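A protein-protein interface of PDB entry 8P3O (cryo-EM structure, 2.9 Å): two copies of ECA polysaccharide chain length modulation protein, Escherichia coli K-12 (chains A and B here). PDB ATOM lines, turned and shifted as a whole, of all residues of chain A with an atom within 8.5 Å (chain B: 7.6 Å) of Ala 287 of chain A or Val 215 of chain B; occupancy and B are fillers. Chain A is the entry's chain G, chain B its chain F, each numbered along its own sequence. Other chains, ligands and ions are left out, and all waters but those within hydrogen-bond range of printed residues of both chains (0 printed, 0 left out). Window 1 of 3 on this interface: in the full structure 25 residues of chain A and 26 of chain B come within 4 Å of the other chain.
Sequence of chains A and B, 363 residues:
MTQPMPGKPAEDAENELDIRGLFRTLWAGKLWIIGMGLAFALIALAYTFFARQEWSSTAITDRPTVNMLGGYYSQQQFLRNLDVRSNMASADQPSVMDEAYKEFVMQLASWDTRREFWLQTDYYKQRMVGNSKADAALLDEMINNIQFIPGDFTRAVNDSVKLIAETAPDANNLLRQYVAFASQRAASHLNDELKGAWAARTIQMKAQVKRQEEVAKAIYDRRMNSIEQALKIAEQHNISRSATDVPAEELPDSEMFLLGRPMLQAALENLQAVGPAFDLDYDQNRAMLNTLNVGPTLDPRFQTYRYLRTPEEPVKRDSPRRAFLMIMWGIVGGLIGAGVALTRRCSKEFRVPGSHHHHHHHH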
ATOM      1  N   PHE A  78     -13.805 -19.299  18.890  1.00  0.00           N
ATOM      2  CA  PHE A  78     -12.851 -18.638  18.007  1.00  0.00           C
ATOM      3  C   PHE A  78     -11.626 -19.510  17.755  1.00  0.00           C
ATOM      4  O   PHE A  78     -11.139 -19.594  16.621  1.00  0.00           O
ATOM      5  CB  PHE A  78     -12.440 -17.293  18.604  1.00  0.00           C
ATOM      6  CG  PHE A  78     -11.244 -16.675  17.945  1.00  0.00           C
ATOM      7  CD1 PHE A  78     -11.331 -16.163  16.663  1.00  0.00           C
ATOM      8  CD2 PHE A  78     -10.035 -16.600  18.612  1.00  0.00           C
ATOM      9  CE1 PHE A  78     -10.230 -15.592  16.057  1.00  0.00           C
ATOM     10  CE2 PHE A  78      -8.932 -16.029  18.011  1.00  0.00           C
ATOM     11  CZ  PHE A  78      -9.030 -15.524  16.731  1.00  0.00           C
ATOM     12  N   MET A 205       1.714 -19.283  14.914  1.00  0.00           N
ATOM     13  CA  MET A 205       1.444 -18.269  13.902  1.00  0.00           C
ATOM     14  C   MET A 205       2.597 -17.286  13.751  1.00  0.00           C
ATOM     15  O   MET A 205       2.910 -16.874  12.630  1.00  0.00           O
ATOM     16  CB  MET A 205       0.157 -17.515  14.240  1.00  0.00           C
ATOM     17  CG  MET A 205      -0.276 -16.519  13.176  1.00  0.00           C
ATOM     18  SD  MET A 205      -1.232 -17.266  11.843  1.00  0.00           S
ATOM     19  CE  MET A 205      -2.027 -18.619  12.704  1.00  0.00           C
ATOM     20  N   VAL A 209       4.619 -16.631   9.894  1.00  0.00           N
ATOM     21  CA  VAL A 209       4.725 -15.323   9.256  1.00  0.00           C
ATOM     22  C   VAL A 209       6.178 -15.009   8.921  1.00  0.00           C
ATOM     23  O   VAL A 209       6.484 -14.491   7.841  1.00  0.00           O
ATOM     24  CB  VAL A 209       4.097 -14.242  10.155  1.00  0.00           C
ATOM     25  CG1 VAL A 209       4.307 -12.857   9.564  1.00  0.00           C
ATOM     26  CG2 VAL A 209       2.618 -14.522  10.358  1.00  0.00           C
ATOM     27  N   ASP A 279       2.147 -10.770  -1.193  1.00  0.00           N
ATOM     28  CA  ASP A 279       0.856 -11.148  -1.740  1.00  0.00           C
ATOM     29  C   ASP A 279      -0.247 -10.868  -0.719  1.00  0.00           C
ATOM     30  O   ASP A 279      -0.013 -10.292   0.346  1.00  0.00           O
ATOM     31  CB  ASP A 279       0.876 -12.617  -2.159  1.00  0.00           C
ATOM     32  CG  ASP A 279       1.350 -13.531  -1.049  1.00  0.00           C
ATOM     33  OD1 ASP A 279       2.353 -13.189  -0.387  1.00  0.00           O
ATOM     34  OD2 ASP A 279       0.719 -14.586  -0.835  1.00  0.00           O
ATOM     35  N   LEU A 280      -1.472 -11.283  -1.051  1.00  0.00           N
ATOM     36  CA  LEU A 280      -2.602 -11.061  -0.154  1.00  0.00           C
ATOM     37  C   LEU A 280      -2.527 -11.937   1.087  1.00  0.00           C
ATOM     38  O   LEU A 280      -2.905 -11.497   2.178  1.00  0.00           O
ATOM     39  CB  LEU A 280      -3.914 -11.308  -0.898  1.00  0.00           C
ATOM     40  CG  LEU A 280      -5.201 -11.033  -0.118  1.00  0.00           C
ATOM     41  CD1 LEU A 280      -5.370  -9.544   0.137  1.00  0.00           C
ATOM     42  CD2 LEU A 280      -6.405 -11.592  -0.858  1.00  0.00           C
ATOM     43  N   ASP A 281      -2.052 -13.178   0.942  1.00  0.00           N
ATOM     44  CA  ASP A 281      -2.022 -14.101   2.072  1.00  0.00           C
ATOM     45  C   ASP A 281      -1.133 -13.592   3.198  1.00  0.00           C
ATOM     46  O   ASP A 281      -1.418 -13.842   4.373  1.00  0.00           O
ATOM     47  CB  ASP A 281      -1.558 -15.480   1.608  1.00  0.00           C
ATOM     48  CG  ASP A 281      -2.028 -16.590   2.523  1.00  0.00           C
ATOM     49  OD1 ASP A 281      -2.713 -16.288   3.522  1.00  0.00           O
ATOM     50  OD2 ASP A 281      -1.714 -17.767   2.244  1.00  0.00           O
ATOM     51  N   TYR A 282      -0.051 -12.887   2.862  1.00  0.00           N
ATOM     52  CA  TYR A 282       0.808 -12.319   3.897  1.00  0.00           C
ATOM     53  C   TYR A 282       0.068 -11.274   4.722  1.00  0.00           C
ATOM     54  O   TYR A 282       0.220 -11.224   5.947  1.00  0.00           O
ATOM     55  CB  TYR A 282       2.060 -11.713   3.265  1.00  0.00           C
ATOM     56  CG  TYR A 282       2.929 -10.947   4.234  1.00  0.00           C
ATOM     57  CD1 TYR A 282       3.770 -11.609   5.118  1.00  0.00           C
ATOM     58  CD2 TYR A 282       2.908  -9.560   4.265  1.00  0.00           C
ATOM     59  CE1 TYR A 282       4.565 -10.912   6.004  1.00  0.00           C
ATOM     60  CE2 TYR A 282       3.700  -8.854   5.147  1.00  0.00           C
ATOM     61  CZ  TYR A 282       4.526  -9.534   6.015  1.00  0.00           C
ATOM     62  OH  TYR A 282       5.316  -8.833   6.894  1.00  0.00           O
ATOM     63  N   ASP A 283      -0.734 -10.430   4.069  1.00  0.00           N
ATOM     64  CA  ASP A 283      -1.421  -9.361   4.785  1.00  0.00           C
ATOM     65  C   ASP A 283      -2.499  -9.896   5.716  1.00  0.00           C
ATOM     66  O   ASP A 283      -2.697  -9.350   6.807  1.00  0.00           O
ATOM     67  CB  ASP A 283      -2.023  -8.368   3.792  1.00  0.00           C
ATOM     68  CG  ASP A 283      -1.018  -7.342   3.315  1.00  0.00           C
ATOM     69  OD1 ASP A 283      -0.582  -6.506   4.136  1.00  0.00           O
ATOM     70  OD2 ASP A 283      -0.659  -7.370   2.118  1.00  0.00           O
ATOM     71  N   GLN A 284      -3.211 -10.948   5.305  1.00  0.00           N
ATOM     72  CA  GLN A 284      -4.253 -11.509   6.157  1.00  0.00           C
ATOM     73  C   GLN A 284      -3.682 -12.082   7.447  1.00  0.00           C
ATOM     74  O   GLN A 284      -4.281 -11.916   8.514  1.00  0.00           O
ATOM     75  CB  GLN A 284      -5.033 -12.584   5.400  1.00  0.00           C
ATOM     76  CG  GLN A 284      -5.919 -12.039   4.294  1.00  0.00           C
ATOM     77  CD  GLN A 284      -6.534 -13.135   3.451  1.00  0.00           C
ATOM     78  OE1 GLN A 284      -6.215 -14.313   3.614  1.00  0.00           O
ATOM     79  NE2 GLN A 284      -7.423 -12.754   2.542  1.00  0.00           N
ATOM     80  N   ASN A 285      -2.533 -12.758   7.370  1.00  0.00           N
ATOM     81  CA  ASN A 285      -1.923 -13.329   8.566  1.00  0.00           C
ATOM     82  C   ASN A 285      -1.507 -12.252   9.559  1.00  0.00           C
ATOM     83  O   ASN A 285      -1.662 -12.439  10.771  1.00  0.00           O
ATOM     84  CB  ASN A 285      -0.723 -14.188   8.182  1.00  0.00           C
ATOM     85  CG  ASN A 285      -1.128 -15.491   7.528  1.00  0.00           C
ATOM     86  OD1 ASN A 285      -2.306 -15.851   7.517  1.00  0.00           O
ATOM     87  ND2 ASN A 285      -0.157 -16.202   6.972  1.00  0.00           N
ATOM     88  N   ARG A 286      -0.969 -11.133   9.074  1.00  0.00           N
ATOM     89  CA  ARG A 286      -0.583 -10.047   9.966  1.00  0.00           C
ATOM     90  C   ARG A 286      -1.780  -9.460  10.702  1.00  0.00           C
ATOM     91  O   ARG A 286      -1.674  -9.147  11.893  1.00  0.00           O
ATOM     92  CB  ARG A 286       0.135  -8.949   9.182  1.00  0.00           C
ATOM     93  CG  ARG A 286       1.356  -9.428   8.423  1.00  0.00           C
ATOM     94  CD  ARG A 286       2.634  -9.043   9.143  1.00  0.00           C
ATOM     95  NE  ARG A 286       2.801  -7.597   9.214  1.00  0.00           N
ATOM     96  CZ  ARG A 286       3.622  -6.980  10.054  1.00  0.00           C
ATOM     97  NH1 ARG A 286       4.365  -7.656  10.915  1.00  0.00           N
ATOM     98  NH2 ARG A 286       3.698  -5.652  10.029  1.00  0.00           N
ATOM     99  N   ALA A 287      -2.912  -9.292  10.016  1.00  0.00           N
ATOM    100  CA  ALA A 287      -4.103  -8.773  10.679  1.00  0.00           C
ATOM    101  C   ALA A 287      -4.611  -9.729  11.750  1.00  0.00           C
ATOM    102  O   ALA A 287      -5.002  -9.288  12.836  1.00  0.00           O
ATOM    103  CB  ALA A 287      -5.199  -8.496   9.653  1.00  0.00           C
ATOM    104  N   MET A 288      -4.617 -11.033  11.465  1.00  0.00           N
ATOM    105  CA  MET A 288      -5.022 -12.013  12.464  1.00  0.00           C
ATOM    106  C   MET A 288      -4.070 -12.038  13.652  1.00  0.00           C
ATOM    107  O   MET A 288      -4.519 -12.154  14.797  1.00  0.00           O
ATOM    108  CB  MET A 288      -5.113 -13.401  11.829  1.00  0.00           C
ATOM    109  CG  MET A 288      -5.243 -14.536  12.828  1.00  0.00           C
ATOM    110  SD  MET A 288      -6.959 -14.889  13.243  1.00  0.00           S
ATOM    111  CE  MET A 288      -7.680 -15.029  11.610  1.00  0.00           C
ATOM    112  N   LEU A 289      -2.765 -11.926  13.400  1.00  0.00           N
ATOM    113  CA  LEU A 289      -1.781 -11.946  14.474  1.00  0.00           C
ATOM    114  C   LEU A 289      -1.968 -10.797  15.455  1.00  0.00           C
ATOM    115  O   LEU A 289      -1.614 -10.940  16.630  1.00  0.00           O
ATOM    116  CB  LEU A 289      -0.369 -11.902  13.886  1.00  0.00           C
ATOM    117  CG  LEU A 289       0.799 -12.087  14.853  1.00  0.00           C
ATOM    118  CD1 LEU A 289       0.692 -13.424  15.562  1.00  0.00           C
ATOM    119  CD2 LEU A 289       2.125 -11.963  14.123  1.00  0.00           C
ATOM    120  N   ASN A 290      -2.514  -9.665  15.005  1.00  0.00           N
ATOM    121  CA  ASN A 290      -2.740  -8.546  15.913  1.00  0.00           C
ATOM    122  C   ASN A 290      -3.761  -8.888  16.989  1.00  0.00           C
ATOM    123  O   ASN A 290      -3.570  -8.535  18.158  1.00  0.00           O
ATOM    124  CB  ASN A 290      -3.193  -7.316  15.128  1.00  0.00           C
ATOM    125  CG  ASN A 290      -2.040  -6.582  14.483  1.00  0.00           C
ATOM    126  OD1 ASN A 290      -0.879  -6.792  14.836  1.00  0.00           O
ATOM    127  ND2 ASN A 290      -2.349  -5.712  13.529  1.00  0.00           N
ATOM    128  N   THR A 291      -4.846  -9.571  16.621  1.00  0.00           N
ATOM    129  CA  THR A 291      -5.852  -9.957  17.603  1.00  0.00           C
ATOM    130  C   THR A 291      -5.300 -10.963  18.606  1.00  0.00           C
ATOM    131  O   THR A 291      -5.594 -10.874  19.803  1.00  0.00           O
ATOM    132  CB  THR A 291      -7.083 -10.533  16.904  1.00  0.00           C
ATOM    133  OG1 THR A 291      -6.906 -11.941  16.706  1.00  0.00           O
ATOM    134  CG2 THR A 291      -7.290  -9.858  15.559  1.00  0.00           C
ATOM    135  N   LEU A 292      -4.508 -11.930  18.137  1.00  0.00           N
ATOM    136  CA  LEU A 292      -3.913 -12.909  19.037  1.00  0.00           C
ATOM    137  C   LEU A 292      -2.959 -12.273  20.039  1.00  0.00           C
ATOM    138  O   LEU A 292      -2.812 -12.792  21.150  1.00  0.00           O
ATOM    139  CB  LEU A 292      -3.186 -13.987  18.234  1.00  0.00           C
ATOM    140  CG  LEU A 292      -4.069 -15.071  17.614  1.00  0.00           C
ATOM    141  CD1 LEU A 292      -3.267 -15.925  16.653  1.00  0.00           C
ATOM    142  CD2 LEU A 292      -4.692 -15.930  18.699  1.00  0.00           C
ATOM    143  N   ASN A 293      -2.313 -11.165  19.676  1.00  0.00           N
ATOM    144  CA  ASN A 293      -1.402 -10.494  20.594  1.00  0.00           C
ATOM    145  C   ASN A 293      -2.128  -9.786  21.729  1.00  0.00           C
ATOM    146  O   ASN A 293      -1.506  -9.493  22.757  1.00  0.00           O
ATOM    147  CB  ASN A 293      -0.536  -9.489  19.833  1.00  0.00           C
ATOM    148  CG  ASN A 293       0.724 -10.113  19.275  1.00  0.00           C
ATOM    149  OD1 ASN A 293       1.087 -11.233  19.635  1.00  0.00           O
ATOM    150  ND2 ASN A 293       1.399  -9.394  18.387  1.00  0.00           N
ATOM    151  N   GLN B 208     -14.769 -10.065  11.894  1.00  0.00           N
ATOM    152  CA  GLN B 208     -14.214 -10.239  10.556  1.00  0.00           C
ATOM    153  C   GLN B 208     -14.347  -8.975   9.720  1.00  0.00           C
ATOM    154  O   GLN B 208     -13.463  -8.675   8.908  1.00  0.00           O
ATOM    155  CB  GLN B 208     -14.890 -11.412   9.849  1.00  0.00           C
ATOM    156  CG  GLN B 208     -15.444 -12.466  10.785  1.00  0.00           C
ATOM    157  CD  GLN B 208     -16.076 -13.621  10.038  1.00  0.00           C
ATOM    158  OE1 GLN B 208     -16.076 -13.653   8.808  1.00  0.00           O
ATOM    159  NE2 GLN B 208     -16.623 -14.577  10.778  1.00  0.00           N
ATOM    160  N   VAL B 209     -15.440  -8.232   9.889  1.00  0.00           N
ATOM    161  CA  VAL B 209     -15.617  -6.987   9.149  1.00  0.00           C
ATOM    162  C   VAL B 209     -14.512  -6.000   9.502  1.00  0.00           C
ATOM    163  O   VAL B 209     -13.947  -5.337   8.624  1.00  0.00           O
ATOM    164  CB  VAL B 209     -17.017  -6.402   9.416  1.00  0.00           C
ATOM    165  CG1 VAL B 209     -17.012  -4.889   9.261  1.00  0.00           C
ATOM    166  CG2 VAL B 209     -18.037  -7.034   8.486  1.00  0.00           C
ATOM    167  N   LYS B 210     -14.181  -5.892  10.791  1.00  0.00           N
ATOM    168  CA  LYS B 210     -13.090  -5.014  11.204  1.00  0.00           C
ATOM    169  C   LYS B 210     -11.758  -5.477  10.628  1.00  0.00           C
ATOM    170  O   LYS B 210     -10.948  -4.654  10.187  1.00  0.00           O
ATOM    171  CB  LYS B 210     -13.021  -4.946  12.728  1.00  0.00           C
ATOM    172  CG  LYS B 210     -13.713  -3.733  13.327  1.00  0.00           C
ATOM    173  CD  LYS B 210     -13.120  -3.360  14.679  1.00  0.00           C
ATOM    174  CE  LYS B 210     -11.605  -3.507  14.685  1.00  0.00           C
ATOM    175  NZ  LYS B 210     -10.974  -2.767  15.811  1.00  0.00           N
ATOM    176  N   ARG B 211     -11.509  -6.789  10.630  1.00  0.00           N
ATOM    177  CA  ARG B 211     -10.261  -7.305  10.079  1.00  0.00           C
ATOM    178  C   ARG B 211     -10.156  -7.049   8.581  1.00  0.00           C
ATOM    179  O   ARG B 211      -9.077  -6.700   8.090  1.00  0.00           O
ATOM    180  CB  ARG B 211     -10.134  -8.799  10.369  1.00  0.00           C
ATOM    181  CG  ARG B 211      -9.520  -9.114  11.721  1.00  0.00           C
ATOM    182  CD  ARG B 211      -8.868 -10.486  11.725  1.00  0.00           C
ATOM    183  NE  ARG B 211      -9.833 -11.552  11.485  1.00  0.00           N
ATOM    184  CZ  ARG B 211     -10.623 -12.071  12.415  1.00  0.00           C
ATOM    185  NH1 ARG B 211     -10.596 -11.636  13.665  1.00  0.00           N
ATOM    186  NH2 ARG B 211     -11.459 -13.048  12.085  1.00  0.00           N
ATOM    187  N   GLN B 212     -11.255  -7.218   7.843  1.00  0.00           N
ATOM    188  CA  GLN B 212     -11.218  -6.982   6.404  1.00  0.00           C
ATOM    189  C   GLN B 212     -10.987  -5.513   6.079  1.00  0.00           C
ATOM    190  O   GLN B 212     -10.392  -5.196   5.042  1.00  0.00           O
ATOM    191  CB  GLN B 212     -12.515  -7.466   5.758  1.00  0.00           C
ATOM    192  CG  GLN B 212     -12.590  -8.971   5.573  1.00  0.00           C
ATOM    193  CD  GLN B 212     -13.929  -9.422   5.025  1.00  0.00           C
ATOM    194  OE1 GLN B 212     -14.955  -8.784   5.258  1.00  0.00           O
ATOM    195  NE2 GLN B 212     -13.925 -10.527   4.289  1.00  0.00           N
ATOM    196  N   GLU B 213     -11.448  -4.606   6.941  1.00  0.00           N
ATOM    197  CA  GLU B 213     -11.254  -3.182   6.687  1.00  0.00           C
ATOM    198  C   GLU B 213      -9.790  -2.780   6.805  1.00  0.00           C
ATOM    199  O   GLU B 213      -9.295  -2.007   5.978  1.00  0.00           O
ATOM    200  CB  GLU B 213     -12.108  -2.357   7.649  1.00  0.00           C
ATOM    201  CG  GLU B 213     -13.384  -1.812   7.035  1.00  0.00           C
ATOM    202  CD  GLU B 213     -14.474  -1.588   8.063  1.00  0.00           C
ATOM    203  OE1 GLU B 213     -14.141  -1.374   9.247  1.00  0.00           O
ATOM    204  OE2 GLU B 213     -15.665  -1.626   7.689  1.00  0.00           O
ATOM    205  N   GLU B 214      -9.083  -3.289   7.813  1.00  0.00           N
ATOM    206  CA  GLU B 214      -7.685  -2.938   8.010  1.00  0.00           C
ATOM    207  C   GLU B 214      -6.751  -3.649   7.043  1.00  0.00           C
ATOM    208  O   GLU B 214      -5.626  -3.180   6.834  1.00  0.00           O
ATOM    209  CB  GLU B 214      -7.258  -3.241   9.451  1.00  0.00           C
ATOM    210  CG  GLU B 214      -6.892  -4.692   9.707  1.00  0.00           C
ATOM    211  CD  GLU B 214      -6.207  -4.892  11.045  1.00  0.00           C
ATOM    212  OE1 GLU B 214      -4.970  -4.729  11.112  1.00  0.00           O
ATOM    213  OE2 GLU B 214      -6.904  -5.207  12.030  1.00  0.00           O
ATOM    214  N   VAL B 215      -7.183  -4.764   6.452  1.00  0.00           N
ATOM    215  CA  VAL B 215      -6.378  -5.411   5.424  1.00  0.00           C
ATOM    216  C   VAL B 215      -6.358  -4.569   4.155  1.00  0.00           C
ATOM    217  O   VAL B 215      -5.304  -4.366   3.543  1.00  0.00           O
ATOM    218  CB  VAL B 215      -6.900  -6.833   5.155  1.00  0.00           C
ATOM    219  CG1 VAL B 215      -6.416  -7.337   3.805  1.00  0.00           C
ATOM    220  CG2 VAL B 215      -6.466  -7.774   6.263  1.00  0.00           C
ATOM    221  N   ALA B 216      -7.522  -4.059   3.746  1.00  0.00           N
ATOM    222  CA  ALA B 216      -7.596  -3.262   2.526  1.00  0.00           C
ATOM    223  C   ALA B 216      -6.843  -1.947   2.661  1.00  0.00           C
ATOM    224  O   ALA B 216      -6.276  -1.457   1.678  1.00  0.00           O
ATOM    225  CB  ALA B 216      -9.056  -3.002   2.158  1.00  0.00           C
ATOM    226  N   LYS B 217      -6.829  -1.359   3.859  1.00  0.00           N
ATOM    227  CA  LYS B 217      -6.098  -0.112   4.060  1.00  0.00           C
ATOM    228  C   LYS B 217      -4.594  -0.312   3.934  1.00  0.00           C
ATOM    229  O   LYS B 217      -3.900   0.554   3.388  1.00  0.00           O
ATOM    230  CB  LYS B 217      -6.436   0.487   5.423  1.00  0.00           C
ATOM    231  CG  LYS B 217      -5.801   1.844   5.669  1.00  0.00           C
ATOM    232  CD  LYS B 217      -5.982   2.291   7.109  1.00  0.00           C
ATOM    233  CE  LYS B 217      -5.339   3.647   7.347  1.00  0.00           C
ATOM    234  NZ  LYS B 217      -5.544   4.120   8.743  1.00  0.00           N
ATOM    235  N   ALA B 218      -4.073  -1.435   4.436  1.00  0.00           N
ATOM    236  CA  ALA B 218      -2.638  -1.685   4.352  1.00  0.00           C
ATOM    237  C   ALA B 218      -2.175  -1.782   2.907  1.00  0.00           C
ATOM    238  O   ALA B 218      -1.122  -1.245   2.545  1.00  0.00           O
ATOM    239  CB  ALA B 218      -2.283  -2.959   5.117  1.00  0.00           C
ATOM    240  N   ILE B 219      -2.948  -2.469   2.064  1.00  0.00           N
ATOM    241  CA  ILE B 219      -2.604  -2.561   0.648  1.00  0.00           C
ATOM    242  C   ILE B 219      -2.670  -1.189  -0.009  1.00  0.00           C
ATOM    243  O   ILE B 219      -1.805  -0.831  -0.817  1.00  0.00           O
ATOM    244  CB  ILE B 219      -3.525  -3.574  -0.056  1.00  0.00           C
ATOM    245  CG1 ILE B 219      -3.302  -4.976   0.509  1.00  0.00           C
ATOM    246  CG2 ILE B 219      -3.284  -3.561  -1.554  1.00  0.00           C
ATOM    247  CD1 ILE B 219      -4.182  -6.032  -0.117  1.00  0.00           C
ATOM    248  N   TYR B 220      -3.692  -0.400   0.327  1.00  0.00           N
ATOM    249  CA  TYR B 220      -3.841   0.923  -0.274  1.00  0.00           C
ATOM    250  C   TYR B 220      -2.674   1.833   0.090  1.00  0.00           C
ATOM    251  O   TYR B 220      -2.182   2.588  -0.757  1.00  0.00           O
ATOM    252  CB  TYR B 220      -5.169   1.542   0.158  1.00  0.00           C
ATOM    253  CG  TYR B 220      -5.271   3.034  -0.069  1.00  0.00           C
ATOM    254  CD1 TYR B 220      -5.633   3.542  -1.308  1.00  0.00           C
ATOM    255  CD2 TYR B 220      -5.021   3.932   0.959  1.00  0.00           C
ATOM    256  CE1 TYR B 220      -5.732   4.903  -1.520  1.00  0.00           C
ATOM    257  CE2 TYR B 220      -5.117   5.293   0.758  1.00  0.00           C
ATOM    258  CZ  TYR B 220      -5.473   5.773  -0.482  1.00  0.00           C
ATOM    259  OH  TYR B 220      -5.570   7.131  -0.685  1.00  0.00           O
ATOM    260  N   ASP B 221      -2.222   1.782   1.345  1.00  0.00           N
ATOM    261  CA  ASP B 221      -1.092   2.609   1.757  1.00  0.00           C
ATOM    262  C   ASP B 221       0.187   2.223   1.026  1.00  0.00           C
ATOM    263  O   ASP B 221       0.972   3.100   0.651  1.00  0.00           O
ATOM    264  CB  ASP B 221      -0.888   2.508   3.268  1.00  0.00           C
ATOM    265  CG  ASP B 221      -1.792   3.445   4.040  1.00  0.00           C
ATOM    266  OD1 ASP B 221      -2.284   4.425   3.442  1.00  0.00           O
ATOM    267  OD2 ASP B 221      -2.008   3.206   5.247  1.00  0.00           O
ATOM    268  N   ARG B 222       0.416   0.923   0.825  1.00  0.00           N
ATOM    269  CA  ARG B 222       1.605   0.480   0.106  1.00  0.00           C
ATOM    270  C   ARG B 222       1.612   0.974  -1.334  1.00  0.00           C
ATOM    271  O   ARG B 222       2.661   1.384  -1.842  1.00  0.00           O
ATOM    272  CB  ARG B 222       1.701  -1.044   0.151  1.00  0.00           C
ATOM    273  CG  ARG B 222       2.847  -1.624  -0.656  1.00  0.00           C
ATOM    274  CD  ARG B 222       2.845  -3.141  -0.592  1.00  0.00           C
ATOM    275  NE  ARG B 222       2.607  -3.628   0.762  1.00  0.00           N
ATOM    276  CZ  ARG B 222       1.910  -4.716   1.056  1.00  0.00           C
ATOM    277  NH1 ARG B 222       1.361  -5.463   0.110  1.00  0.00           N
ATOM    278  NH2 ARG B 222       1.758  -5.065   2.330  1.00  0.00           N
ATOM    279  N   PRO B 276      -9.580   3.008  -0.830  1.00  0.00           N
ATOM    280  CA  PRO B 276      -9.407   1.561  -0.671  1.00  0.00           C
ATOM    281  C   PRO B 276     -10.426   0.782  -1.489  1.00  0.00           C
ATOM    282  O   PRO B 276     -11.573   1.197  -1.656  1.00  0.00           O
ATOM    283  CB  PRO B 276      -9.612   1.340   0.833  1.00  0.00           C
ATOM    284  CG  PRO B 276      -9.353   2.673   1.454  1.00  0.00           C
ATOM    285  CD  PRO B 276      -9.824   3.682   0.455  1.00  0.00           C
ATOM    286  N   ALA B 277      -9.986  -0.363  -2.005  1.00  0.00           N
ATOM    287  CA  ALA B 277     -10.803  -1.209  -2.863  1.00  0.00           C
ATOM    288  C   ALA B 277     -11.182  -2.480  -2.119  1.00  0.00           C
ATOM    289  O   ALA B 277     -10.312  -3.187  -1.599  1.00  0.00           O
ATOM    290  CB  ALA B 277     -10.061  -1.555  -4.155  1.00  0.00           C
ATOM    291  N   PHE B 278     -12.479  -2.769  -2.071  1.00  0.00           N
ATOM    292  CA  PHE B 278     -13.002  -3.965  -1.434  1.00  0.00           C
ATOM    293  C   PHE B 278     -13.540  -4.926  -2.483  1.00  0.00           C
ATOM    294  O   PHE B 278     -13.889  -4.534  -3.601  1.00  0.00           O
ATOM    295  CB  PHE B 278     -14.107  -3.616  -0.431  1.00  0.00           C
ATOM    296  CG  PHE B 278     -13.709  -2.576   0.572  1.00  0.00           C
ATOM    297  CD1 PHE B 278     -13.037  -2.933   1.727  1.00  0.00           C
ATOM    298  CD2 PHE B 278     -14.010  -1.241   0.363  1.00  0.00           C
ATOM    299  CE1 PHE B 278     -12.671  -1.980   2.655  1.00  0.00           C
ATOM    300  CE2 PHE B 278     -13.646  -0.283   1.287  1.00  0.00           C
ATOM    301  CZ  PHE B 278     -12.976  -0.654   2.435  1.00  0.00           C
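CD1 of Ile 219 of chain B touches CD1 of Leu 280 of chain A, at 3.7 Å.
OD2 of Asp 283 of chain A touches CG1 of Ile 219 of chain B (3.9 Å).
Ala 287 of chain A touches Glu 214 of chain B (CB to CD, 3.99 Å).
Ala 287 of chain A touches Val 215 of chain B.
ND2 of Asn 290 of chain A touches OE1 of Glu 214 of chain B, 3.7 Å away.
1 position is printed for both chains.
Hydrophobic or aromatic side chains of chain B that line the printed part of chain A: Val 215 and Ile 219.
Of the 18 printed residues of chain A, 4 touch a printed residue of chain B.
Hydrophobic or aromatic side chains of chain A that line the printed part of chain B: Leu 280 and Ala 287.
Along chain A the printed residues that touch a printed residue of chain B span positions 280 to 290.
The side-chain carboxylate (OD1) of Asp 283 of chain A is in salt-bridge range of the guanidinium group (NH2) of Arg 222 of chain B (3.3 Å).
Of the printed residues of chain B, Leu 280 of chain A touches Ile 219.
Of the printed residues of chain B, Asp 283 of chain A touches Ile 219 and Arg 222.
Of the printed residues of chain B, Ala 287 of chain A touches Glu 214 and Val 215.
Leu 289 of chain A touches none of the printed residues of chain B.
Of the printed residues of chain A, Glu 214 of chain B touches Ala 287 (3.99 Å) and Asn 290 (3.7 Å).
Val 215 of chain B touches just one residue of chain A: Ala 287 (3.7 Å).
Printed residues of chain A within 4 Å of Ile 219 of chain B: Leu 280 and Asp 283.
The nearest printed residue of chain B that does not touch Ala 287 of chain A is Arg 211 of chain B (4.2 Å).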
